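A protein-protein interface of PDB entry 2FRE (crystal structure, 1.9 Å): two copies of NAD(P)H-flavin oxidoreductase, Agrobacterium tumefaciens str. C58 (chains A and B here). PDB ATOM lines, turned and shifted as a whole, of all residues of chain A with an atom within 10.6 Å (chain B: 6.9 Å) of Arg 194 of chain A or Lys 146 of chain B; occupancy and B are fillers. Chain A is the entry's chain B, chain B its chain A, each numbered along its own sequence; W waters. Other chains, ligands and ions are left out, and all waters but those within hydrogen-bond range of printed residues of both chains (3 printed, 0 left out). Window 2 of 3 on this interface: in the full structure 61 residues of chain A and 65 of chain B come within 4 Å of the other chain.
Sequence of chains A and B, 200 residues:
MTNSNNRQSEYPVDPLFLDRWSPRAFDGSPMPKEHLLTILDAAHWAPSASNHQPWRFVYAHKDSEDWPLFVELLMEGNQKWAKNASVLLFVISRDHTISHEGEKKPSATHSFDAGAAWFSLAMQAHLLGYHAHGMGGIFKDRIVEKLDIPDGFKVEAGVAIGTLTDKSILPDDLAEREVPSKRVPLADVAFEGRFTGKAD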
ATOM      1  N   ALA A 187       5.421  13.282 -15.732  1.00  0.00           N
ATOM      2  CA  ALA A 187       3.969  13.444 -15.850  1.00  0.00           C
ATOM      3  C   ALA A 187       3.197  12.131 -15.772  1.00  0.00           C
ATOM      4  O   ALA A 187       1.986  12.144 -15.572  1.00  0.00           O
ATOM      5  CB  ALA A 187       3.625  14.176 -17.115  1.00  0.00           C
ATOM      6  N   ASP A 188       3.895  11.006 -15.931  1.00  0.00           N
ATOM      7  CA  ASP A 188       3.307   9.680 -15.784  1.00  0.00           C
ATOM      8  C   ASP A 188       3.138   9.258 -14.326  1.00  0.00           C
ATOM      9  O   ASP A 188       2.398   8.325 -14.048  1.00  0.00           O
ATOM     10  CB  ASP A 188       4.154   8.628 -16.498  1.00  0.00           C
ATOM     11  CG  ASP A 188       4.038   8.702 -17.999  1.00  0.00           C
ATOM     12  OD1 ASP A 188       3.349   9.594 -18.523  1.00  0.00           O
ATOM     13  OD2 ASP A 188       4.632   7.832 -18.659  1.00  0.00           O
ATOM     14  N   VAL A 189       3.823   9.930 -13.398  1.00  0.00           N
ATOM     15  CA  VAL A 189       3.697   9.611 -11.975  1.00  0.00           C
ATOM     16  C   VAL A 189       3.314  10.786 -11.060  1.00  0.00           C
ATOM     17  O   VAL A 189       2.951  10.551  -9.905  1.00  0.00           O
ATOM     18  CB  VAL A 189       4.996   8.950 -11.400  1.00  0.00           C
ATOM     19  CG1 VAL A 189       5.319   7.684 -12.157  1.00  0.00           C
ATOM     20  CG2 VAL A 189       6.179   9.912 -11.413  1.00  0.00           C
ATOM     21  N   ALA A 190       3.404  12.023 -11.565  1.00  0.00           N
ATOM     22  CA  ALA A 190       3.062  13.220 -10.805  1.00  0.00           C
ATOM     23  C   ALA A 190       1.828  13.890 -11.396  1.00  0.00           C
ATOM     24  O   ALA A 190       1.823  14.313 -12.558  1.00  0.00           O
ATOM     25  CB  ALA A 190       4.250  14.198 -10.772  1.00  0.00           C
ATOM     26  N   PHE A 191       0.767  13.965 -10.595  1.00  0.00           N
ATOM     27  CA  PHE A 191      -0.514  14.470 -11.059  1.00  0.00           C
ATOM     28  C   PHE A 191      -0.978  15.657 -10.224  1.00  0.00           C
ATOM     29  O   PHE A 191      -1.035  15.572  -9.000  1.00  0.00           O
ATOM     30  CB  PHE A 191      -1.563  13.373 -10.970  1.00  0.00           C
ATOM     31  CG  PHE A 191      -1.097  12.040 -11.485  1.00  0.00           C
ATOM     32  CD1 PHE A 191      -0.527  11.927 -12.749  1.00  0.00           C
ATOM     33  CD2 PHE A 191      -1.237  10.911 -10.719  1.00  0.00           C
ATOM     34  CE1 PHE A 191      -0.114  10.709 -13.230  1.00  0.00           C
ATOM     35  CE2 PHE A 191      -0.823   9.680 -11.202  1.00  0.00           C
ATOM     36  CZ  PHE A 191      -0.256   9.592 -12.461  1.00  0.00           C
ATOM     37  N   GLU A 192      -1.337  16.752 -10.887  1.00  0.00           N
ATOM     38  CA  GLU A 192      -1.871  17.920 -10.201  1.00  0.00           C
ATOM     39  C   GLU A 192      -3.360  17.769  -9.914  1.00  0.00           C
ATOM     40  O   GLU A 192      -4.146  17.430 -10.809  1.00  0.00           O
ATOM     41  CB  GLU A 192      -1.642  19.193 -11.015  1.00  0.00           C
ATOM     42  CG  GLU A 192      -1.852  20.453 -10.195  1.00  0.00           C
ATOM     43  CD  GLU A 192      -1.370  21.729 -10.903  1.00  0.00           C
ATOM     44  OE1 GLU A 192      -1.619  21.871 -12.128  1.00  0.00           O
ATOM     45  OE2 GLU A 192      -0.764  22.600 -10.222  1.00  0.00           O
ATOM     46  N   GLY A 193      -3.754  18.016  -8.669  1.00  0.00           N
ATOM     47  CA  GLY A 193      -5.173  18.152  -8.320  1.00  0.00           C
ATOM     48  C   GLY A 193      -5.894  16.835  -8.061  1.00  0.00           C
ATOM     49  O   GLY A 193      -6.594  16.695  -7.063  1.00  0.00           O
ATOM     50  N   ARG A 194      -5.742  15.881  -8.976  1.00  0.00           N
ATOM     51  CA  ARG A 194      -6.425  14.587  -8.894  1.00  0.00           C
ATOM     52  C   ARG A 194      -5.539  13.526  -9.508  1.00  0.00           C
ATOM     53  O   ARG A 194      -4.722  13.828 -10.376  1.00  0.00           O
ATOM     54  CB  ARG A 194      -7.733  14.620  -9.687  1.00  0.00           C
ATOM     55  CG  ARG A 194      -8.781  15.591  -9.178  1.00  0.00           C
ATOM     56  CD  ARG A 194      -9.454  15.098  -7.909  1.00  0.00           C
ATOM     57  NE  ARG A 194     -10.664  15.875  -7.628  1.00  0.00           N
ATOM     58  CZ  ARG A 194     -10.675  17.076  -7.049  1.00  0.00           C
ATOM     59  NH1 ARG A 194      -9.538  17.660  -6.671  1.00  0.00           N
ATOM     60  NH2 ARG A 194     -11.828  17.705  -6.847  1.00  0.00           N
ATOM     61  N   PHE A 195      -5.723  12.278  -9.087  1.00  0.00           N
ATOM     62  CA  PHE A 195      -5.026  11.159  -9.724  1.00  0.00           C
ATOM     63  C   PHE A 195      -5.587  10.999 -11.135  1.00  0.00           C
ATOM     64  O   PHE A 195      -6.774  10.704 -11.304  1.00  0.00           O
ATOM     65  CB  PHE A 195      -5.224   9.875  -8.903  1.00  0.00           C
ATOM     66  CG  PHE A 195      -4.305   8.739  -9.295  1.00  0.00           C
ATOM     67  CD1 PHE A 195      -3.335   8.286  -8.422  1.00  0.00           C
ATOM     68  CD2 PHE A 195      -4.430   8.108 -10.525  1.00  0.00           C
ATOM     69  CE1 PHE A 195      -2.494   7.230  -8.777  1.00  0.00           C
ATOM     70  CE2 PHE A 195      -3.590   7.054 -10.885  1.00  0.00           C
ATOM     71  CZ  PHE A 195      -2.623   6.619 -10.002  1.00  0.00           C
ATOM     72  N   THR A 196      -4.735  11.209 -12.142  1.00  0.00           N
ATOM     73  CA  THR A 196      -5.149  11.163 -13.548  1.00  0.00           C
ATOM     74  C   THR A 196      -4.365  10.158 -14.383  1.00  0.00           C
ATOM     75  O   THR A 196      -4.526  10.103 -15.603  1.00  0.00           O
ATOM     76  CB  THR A 196      -4.986  12.541 -14.231  1.00  0.00           C
ATOM     77  OG1 THR A 196      -3.650  13.015 -14.050  1.00  0.00           O
ATOM     78  CG2 THR A 196      -5.967  13.540 -13.673  1.00  0.00           C
ATOM     79  N   GLY A 197      -3.532   9.348 -13.741  1.00  0.00           N
ATOM     80  CA  GLY A 197      -2.628   8.475 -14.473  1.00  0.00           C
ATOM     81  C   GLY A 197      -3.274   7.201 -14.973  1.00  0.00           C
ATOM     82  O   GLY A 197      -4.454   6.956 -14.757  1.00  0.00           O
ATOM     83  N   LYS A 198      -2.453   6.398 -15.645  1.00  0.00           N
ATOM     84  CA  LYS A 198      -2.730   4.997 -16.028  1.00  0.00           C
ATOM     85  C   LYS A 198      -3.038   4.921 -17.512  1.00  0.00           C
ATOM     86  O   LYS A 198      -2.108   4.968 -18.327  1.00  0.00           O
ATOM     87  CB  LYS A 198      -3.814   4.318 -15.176  1.00  0.00           C
ATOM     88  CG  LYS A 198      -3.648   4.480 -13.648  1.00  0.00           C
ATOM     89  CD  LYS A 198      -2.566   3.628 -13.057  1.00  0.00           C
ATOM     90  CE  LYS A 198      -1.122   4.181 -13.203  1.00  0.00           C
ATOM     91  NZ  LYS A 198      -0.854   5.607 -12.994  1.00  0.00           N
ATOM     92  N   PHE B  57       2.367  10.682  -7.180  1.00  0.00           N
ATOM     93  CA  PHE B  57       2.208  11.931  -6.401  1.00  0.00           C
ATOM     94  C   PHE B  57       1.001  12.730  -6.902  1.00  0.00           C
ATOM     95  O   PHE B  57       0.908  13.060  -8.095  1.00  0.00           O
ATOM     96  CB  PHE B  57       3.456  12.790  -6.522  1.00  0.00           C
ATOM     97  CG  PHE B  57       4.717  12.018  -6.327  1.00  0.00           C
ATOM     98  CD1 PHE B  57       5.133  11.664  -5.062  1.00  0.00           C
ATOM     99  CD2 PHE B  57       5.481  11.617  -7.421  1.00  0.00           C
ATOM    100  CE1 PHE B  57       6.282  10.926  -4.878  1.00  0.00           C
ATOM    101  CE2 PHE B  57       6.633  10.849  -7.234  1.00  0.00           C
ATOM    102  CZ  PHE B  57       7.029  10.518  -5.960  1.00  0.00           C
ATOM    103  N   VAL B  58       0.087  13.050  -5.996  1.00  0.00           N
ATOM    104  CA  VAL B  58      -1.038  13.927  -6.327  1.00  0.00           C
ATOM    105  C   VAL B  58      -0.850  15.204  -5.502  1.00  0.00           C
ATOM    106  O   VAL B  58      -0.784  15.161  -4.277  1.00  0.00           O
ATOM    107  CB  VAL B  58      -2.380  13.235  -6.061  1.00  0.00           C
ATOM    108  CG1 VAL B  58      -3.548  14.105  -6.478  1.00  0.00           C
ATOM    109  CG2 VAL B  58      -2.412  11.903  -6.832  1.00  0.00           C
ATOM    110  N   TYR B  59      -0.711  16.326  -6.193  1.00  0.00           N
ATOM    111  CA  TYR B  59      -0.294  17.568  -5.563  1.00  0.00           C
ATOM    112  C   TYR B  59      -1.189  18.768  -5.873  1.00  0.00           C
ATOM    113  O   TYR B  59      -1.908  18.798  -6.878  1.00  0.00           O
ATOM    114  CB  TYR B  59       1.159  17.873  -5.955  1.00  0.00           C
ATOM    115  CG  TYR B  59       1.363  18.196  -7.423  1.00  0.00           C
ATOM    116  CD1 TYR B  59       1.189  19.494  -7.904  1.00  0.00           C
ATOM    117  CD2 TYR B  59       1.717  17.201  -8.330  1.00  0.00           C
ATOM    118  CE1 TYR B  59       1.380  19.791  -9.257  1.00  0.00           C
ATOM    119  CE2 TYR B  59       1.909  17.485  -9.663  1.00  0.00           C
ATOM    120  CZ  TYR B  59       1.732  18.781 -10.118  1.00  0.00           C
ATOM    121  OH  TYR B  59       1.942  19.047 -11.446  1.00  0.00           O
ATOM    122  N   ASP B  66      -8.280  23.583  -5.703  1.00  0.00           N
ATOM    123  CA  ASP B  66      -8.476  22.448  -4.790  1.00  0.00           C
ATOM    124  C   ASP B  66      -7.654  22.462  -3.509  1.00  0.00           C
ATOM    125  O   ASP B  66      -7.651  21.481  -2.779  1.00  0.00           O
ATOM    126  CB  ASP B  66      -8.195  21.144  -5.512  1.00  0.00           C
ATOM    127  CG  ASP B  66      -9.184  20.877  -6.603  1.00  0.00           C
ATOM    128  OD1 ASP B  66     -10.422  20.987  -6.373  1.00  0.00           O
ATOM    129  OD2 ASP B  66      -8.704  20.547  -7.694  1.00  0.00           O
ATOM    130  N   LEU B  69      -9.608  21.449  -0.369  1.00  0.00           N
ATOM    131  CA  LEU B  69      -9.855  20.022  -0.334  1.00  0.00           C
ATOM    132  C   LEU B  69      -8.627  19.287   0.192  1.00  0.00           C
ATOM    133  O   LEU B  69      -8.747  18.388   1.028  1.00  0.00           O
ATOM    134  CB  LEU B  69     -10.237  19.506  -1.714  1.00  0.00           C
ATOM    135  CG  LEU B  69     -10.285  17.975  -1.859  1.00  0.00           C
ATOM    136  CD1 LEU B  69     -11.367  17.339  -0.957  1.00  0.00           C
ATOM    137  CD2 LEU B  69     -10.524  17.657  -3.310  1.00  0.00           C
ATOM    138  N   PHE B  70      -7.453  19.647  -0.311  1.00  0.00           N
ATOM    139  CA  PHE B  70      -6.217  19.022   0.150  1.00  0.00           C
ATOM    140  C   PHE B  70      -6.001  19.270   1.643  1.00  0.00           C
ATOM    141  O   PHE B  70      -5.594  18.376   2.359  1.00  0.00           O
ATOM    142  CB  PHE B  70      -5.014  19.512  -0.666  1.00  0.00           C
ATOM    143  CG  PHE B  70      -4.812  18.762  -1.950  1.00  0.00           C
ATOM    144  CD1 PHE B  70      -5.774  18.775  -2.945  1.00  0.00           C
ATOM    145  CD2 PHE B  70      -3.643  18.030  -2.169  1.00  0.00           C
ATOM    146  CE1 PHE B  70      -5.589  18.050  -4.152  1.00  0.00           C
ATOM    147  CE2 PHE B  70      -3.457  17.318  -3.372  1.00  0.00           C
ATOM    148  CZ  PHE B  70      -4.415  17.327  -4.346  1.00  0.00           C
ATOM    149  N   GLU B  72      -8.405  19.777   3.935  1.00  0.00           N
ATOM    150  CA  GLU B  72      -9.418  19.147   4.790  1.00  0.00           C
ATOM    151  C   GLU B  72      -9.304  17.626   4.789  1.00  0.00           C
ATOM    152  O   GLU B  72      -9.955  16.971   5.603  1.00  0.00           O
ATOM    153  CB  GLU B  72     -10.826  19.629   4.428  1.00  0.00           C
ATOM    154  CG  GLU B  72     -11.410  19.013   3.197  1.00  0.00           C
ATOM    155  CD  GLU B  72     -12.723  19.660   2.795  1.00  0.00           C
ATOM    156  OE1 GLU B  72     -13.659  19.745   3.634  1.00  0.00           O
ATOM    157  OE2 GLU B  72     -12.817  20.065   1.619  1.00  0.00           O
ATOM    158  N   LEU B  73      -8.461  17.091   3.887  1.00  0.00           N
ATOM    159  CA  LEU B  73      -8.092  15.682   3.837  1.00  0.00           C
ATOM    160  C   LEU B  73      -7.023  15.321   4.878  1.00  0.00           C
ATOM    161  O   LEU B  73      -6.735  14.147   5.095  1.00  0.00           O
ATOM    162  CB  LEU B  73      -7.601  15.289   2.442  1.00  0.00           C
ATOM    163  CG  LEU B  73      -8.684  15.212   1.353  1.00  0.00           C
ATOM    164  CD1 LEU B  73      -8.036  14.987  -0.011  1.00  0.00           C
ATOM    165  CD2 LEU B  73      -9.682  14.128   1.665  1.00  0.00           C
ATOM    166  N   ASP B 141      -8.975   6.931   3.349  1.00  0.00           N
ATOM    167  CA  ASP B 141     -10.135   6.518   2.569  1.00  0.00           C
ATOM    168  C   ASP B 141     -10.780   7.702   1.859  1.00  0.00           C
ATOM    169  O   ASP B 141     -11.169   7.582   0.703  1.00  0.00           O
ATOM    170  CB  ASP B 141     -11.149   5.783   3.443  1.00  0.00           C
ATOM    171  CG  ASP B 141     -10.670   4.403   3.852  1.00  0.00           C
ATOM    172  OD1 ASP B 141      -9.711   3.894   3.248  1.00  0.00           O
ATOM    173  OD2 ASP B 141     -11.263   3.809   4.771  1.00  0.00           O
ATOM    174  N   ARG B 142     -10.872   8.848   2.531  1.00  0.00           N
ATOM    175  CA  ARG B 142     -11.392  10.065   1.890  1.00  0.00           C
ATOM    176  C   ARG B 142     -10.452  10.543   0.781  1.00  0.00           C
ATOM    177  O   ARG B 142     -10.908  11.035  -0.252  1.00  0.00           O
ATOM    178  CB  ARG B 142     -11.581  11.210   2.893  1.00  0.00           C
ATOM    179  CG  ARG B 142     -12.463  10.902   4.087  1.00  0.00           C
ATOM    180  CD  ARG B 142     -12.698  12.163   4.913  1.00  0.00           C
ATOM    181  NE  ARG B 142     -13.244  11.844   6.231  1.00  0.00           N
ATOM    182  CZ  ARG B 142     -13.368  12.716   7.228  1.00  0.00           C
ATOM    183  NH1 ARG B 142     -13.000  13.972   7.069  1.00  0.00           N
ATOM    184  NH2 ARG B 142     -13.866  12.328   8.397  1.00  0.00           N
ATOM    185  N   ILE B 143      -9.143  10.432   1.000  1.00  0.00           N
ATOM    186  CA  ILE B 143      -8.173  10.758  -0.049  1.00  0.00           C
ATOM    187  C   ILE B 143      -8.409   9.912  -1.305  1.00  0.00           C
ATOM    188  O   ILE B 143      -8.450  10.433  -2.427  1.00  0.00           O
ATOM    189  CB  ILE B 143      -6.694  10.604   0.467  1.00  0.00           C
ATOM    190  CG1 ILE B 143      -6.390  11.716   1.481  1.00  0.00           C
ATOM    191  CG2 ILE B 143      -5.697  10.649  -0.680  1.00  0.00           C
ATOM    192  CD1 ILE B 143      -5.284  11.364   2.459  1.00  0.00           C
ATOM    193  N   VAL B 144      -8.566   8.605  -1.110  1.00  0.00           N
ATOM    194  CA  VAL B 144      -8.798   7.690  -2.219  1.00  0.00           C
ATOM    195  C   VAL B 144     -10.057   8.057  -3.004  1.00  0.00           C
ATOM    196  O   VAL B 144     -10.052   8.067  -4.229  1.00  0.00           O
ATOM    197  CB  VAL B 144      -8.888   6.215  -1.709  1.00  0.00           C
ATOM    198  CG1 VAL B 144      -9.423   5.279  -2.792  1.00  0.00           C
ATOM    199  CG2 VAL B 144      -7.519   5.756  -1.233  1.00  0.00           C
ATOM    200  N   GLU B 145     -11.124   8.373  -2.287  1.00  0.00           N
ATOM    201  CA  GLU B 145     -12.403   8.695  -2.906  1.00  0.00           C
ATOM    202  C   GLU B 145     -12.354  10.064  -3.584  1.00  0.00           C
ATOM    203  O   GLU B 145     -12.708  10.185  -4.747  1.00  0.00           O
ATOM    204  CB  GLU B 145     -13.504   8.681  -1.851  1.00  0.00           C
ATOM    205  CG  GLU B 145     -14.895   8.878  -2.402  1.00  0.00           C
ATOM    206  CD  GLU B 145     -15.274   7.811  -3.423  1.00  0.00           C
ATOM    207  OE1 GLU B 145     -14.825   6.644  -3.271  1.00  0.00           O
ATOM    208  OE2 GLU B 145     -16.018   8.144  -4.379  1.00  0.00           O
ATOM    209  N   LYS B 146     -11.908  11.089  -2.856  1.00  0.00           N
ATOM    210  CA  LYS B 146     -11.943  12.466  -3.359  1.00  0.00           C
ATOM    211  C   LYS B 146     -10.911  12.754  -4.454  1.00  0.00           C
ATOM    212  O   LYS B 146     -11.129  13.641  -5.282  1.00  0.00           O
ATOM    213  CB  LYS B 146     -11.765  13.476  -2.215  1.00  0.00           C
ATOM    214  CG  LYS B 146     -12.906  13.524  -1.216  1.00  0.00           C
ATOM    215  CD  LYS B 146     -14.154  14.245  -1.744  1.00  0.00           C
ATOM    216  CE  LYS B 146     -15.090  14.619  -0.579  1.00  0.00           C
ATOM    217  NZ  LYS B 146     -16.482  14.970  -0.975  1.00  0.00           N
ATOM    218  N   LEU B 147      -9.786  12.040  -4.449  1.00  0.00           N
ATOM    219  CA  LEU B 147      -8.721  12.287  -5.429  1.00  0.00           C
ATOM    220  C   LEU B 147      -8.679  11.236  -6.538  1.00  0.00           C
ATOM    221  O   LEU B 147      -7.745  11.217  -7.340  1.00  0.00           O
ATOM    222  CB  LEU B 147      -7.346  12.408  -4.744  1.00  0.00           C
ATOM    223  CG  LEU B 147      -7.244  13.506  -3.662  1.00  0.00           C
ATOM    224  CD1 LEU B 147      -5.845  13.660  -3.193  1.00  0.00           C
ATOM    225  CD2 LEU B 147      -7.775  14.881  -4.142  1.00  0.00           C
ATOM    226  N   ASP B 148      -9.703  10.387  -6.586  1.00  0.00           N
ATOM    227  CA  ASP B 148      -9.887   9.415  -7.671  1.00  0.00           C
ATOM    228  C   ASP B 148      -8.718   8.453  -7.771  1.00  0.00           C
ATOM    229  O   ASP B 148      -8.230   8.170  -8.861  1.00  0.00           O
ATOM    230  CB  ASP B 148     -10.075  10.117  -9.020  1.00  0.00           C
ATOM    231  CG  ASP B 148     -11.283  11.027  -9.045  1.00  0.00           C
ATOM    232  OD1 ASP B 148     -12.314  10.648  -8.447  1.00  0.00           O
ATOM    233  OD2 ASP B 148     -11.193  12.123  -9.659  1.00  0.00           O
ATOM    234  N   ILE B 149      -8.263   7.955  -6.629  1.00  0.00           N
ATOM    235  CA  ILE B 149      -7.173   7.014  -6.638  1.00  0.00           C
ATOM    236  C   ILE B 149      -7.752   5.658  -7.015  1.00  0.00           C
ATOM    237  O   ILE B 149      -8.720   5.226  -6.391  1.00  0.00           O
ATOM    238  CB  ILE B 149      -6.466   6.986  -5.288  1.00  0.00           C
ATOM    239  CG1 ILE B 149      -5.798   8.356  -5.066  1.00  0.00           C
ATOM    240  CG2 ILE B 149      -5.441   5.818  -5.237  1.00  0.00           C
ATOM    241  CD1 ILE B 149      -5.372   8.596  -3.681  1.00  0.00           C
HETATM  242  O   HOH W   1       2.808  16.743 -13.055  1.00  0.00           O
HETATM  243  O   HOH W   2     -12.872  14.163  -9.600  1.00  0.00           O
HETATM  244  O   HOH W   3      -8.247   7.867 -11.452  1.00  0.00           O
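Of the 12 printed residues of chain A, 7 touch a printed residue of chain B.
Of the 17 printed residues of chain B, 9 touch a printed residue of chain A.
Hydrophobic or aromatic side chains of chain B within 4 Å of the printed part of chain A: Phe 57, Val 58, Tyr 59, Leu 69, Phe 70 and Leu 147.
No position is printed for both chains.
Of chain B, only Val 58 (3.7 Å), Asp 66 (3.2 Å), Leu 69 (3.5 Å), Lys 146 (3.3 Å), Leu 147 (3.8 Å) and Asp 148 (3.9 Å) come within 4 Å of Arg 194 of chain A.
No residue of chain A comes within 4 Å of Glu 145 of chain B.
Leu 147 of chain B touches just these residues of chain A: Gly 193 (3.6 Å), Arg 194 (3.8 Å) and Phe 195 (2.9 Å).
Of chain A, only Arg 194 and Phe 195 come within 4 Å of Asp 148 of chain B.
Of the printed residues of chain B, Ala 190 of chain A touches Phe 57 and Tyr 59.
Printed residues of chain B within 4 Å of Val 189 of chain A: Phe 57.
Printed residues of chain B within 4 Å of Glu 192 of chain A: Tyr 59.
Printed residues of chain A within 4 Å of Phe 70 of chain B: Gly 193 (3.4 Å).
Printed residues of chain A within 4 Å of Tyr 59 of chain B: Ala 190 (3.99 Å), Phe 191 (2.9 Å), Glu 192 (3.4 Å) and Gly 193 (2.7 Å).
Gly 197 of chain A touches none of the printed residues of chain B.
Glu 72 of chain B touches none of the printed residues of chain A.
The nearest residue of chain A that does not touch Lys 146 of chain B is Gly 193 of chain A (5.8 Å).
The nearest printed residue of chain B that does not touch Gly 193 of chain A is Asp 66 of chain B (4.3 Å).
The backbone NH (N) of Phe 57 of chain B sits at hydrogen-bond distance from the backbone carbonyl oxygen (O) of Val 189 of chain A (2.8 Å).
N of Phe 191 of chain A lies within hydrogen-bond range of O of Phe 57 of chain B (2.7 Å).
The backbone NH (N) of Tyr 59 of chain B sits at hydrogen-bond distance from the backbone carbonyl oxygen (O) of Phe 191 of chain A (2.9 Å).
O of Tyr 59 of chain B is in hydrogen-bond range of N of Gly 193 of chain A, 2.7 Å away.
OD2 of Asp 66 of chain B lies within salt-bridge range of NH1 of Arg 194 of chain A.
The backbone carbonyl oxygen (O) of Lys 146 of chain B lies within hydrogen-bond range of the guanidinium group (NE) of Arg 194 of chain A (3.3 Å).
The backbone NH (N) of Phe 195 of chain A lies within hydrogen-bond range of the backbone carbonyl oxygen (O) of Leu 147 of chain B, at 2.9 Å.
Among the printed residues, merely in contact across the chains: Ala 190 of chain A with Phe 57 of chain B, Ala 190 of chain A with Tyr 59 of chain B, Phe 191 of chain A with Val 58 of chain B, Glu 192 of chain A with Tyr 59 of chain B, Gly 193 of chain A with Val 58 of chain B, Gly 193 of chain A with Phe 70 of chain B, Gly 193 of chain A with Leu 147 of chain B, Arg 194 of chain A with Val 58 of chain B, Arg 194 of chain A with Leu 69 of chain B, Arg 194 of chain A with Leu 147 of chain B, Arg 194 of chain A with Asp 148 of chain B, Phe 195 of chain A with Val 58 of chain B and Phe 195 of chain A with Asp 148 of chain B.
Water W3 bridges the backbone carbonyl oxygen of Asp 148 of chain B (2.6 Å) and the backbone carbonyl oxygen of Phe 195 of chain A (3.2 Å).
Water W2 bridges the side-chain carboxylate of Asp 148 of chain B and the guanidinium group of Arg 194 of chain A.
Water W1 lies within hydrogen-bond range of O of Ala 190 of chain A (2.7 Å) and OH of Tyr 59 of chain B (2.9 Å).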
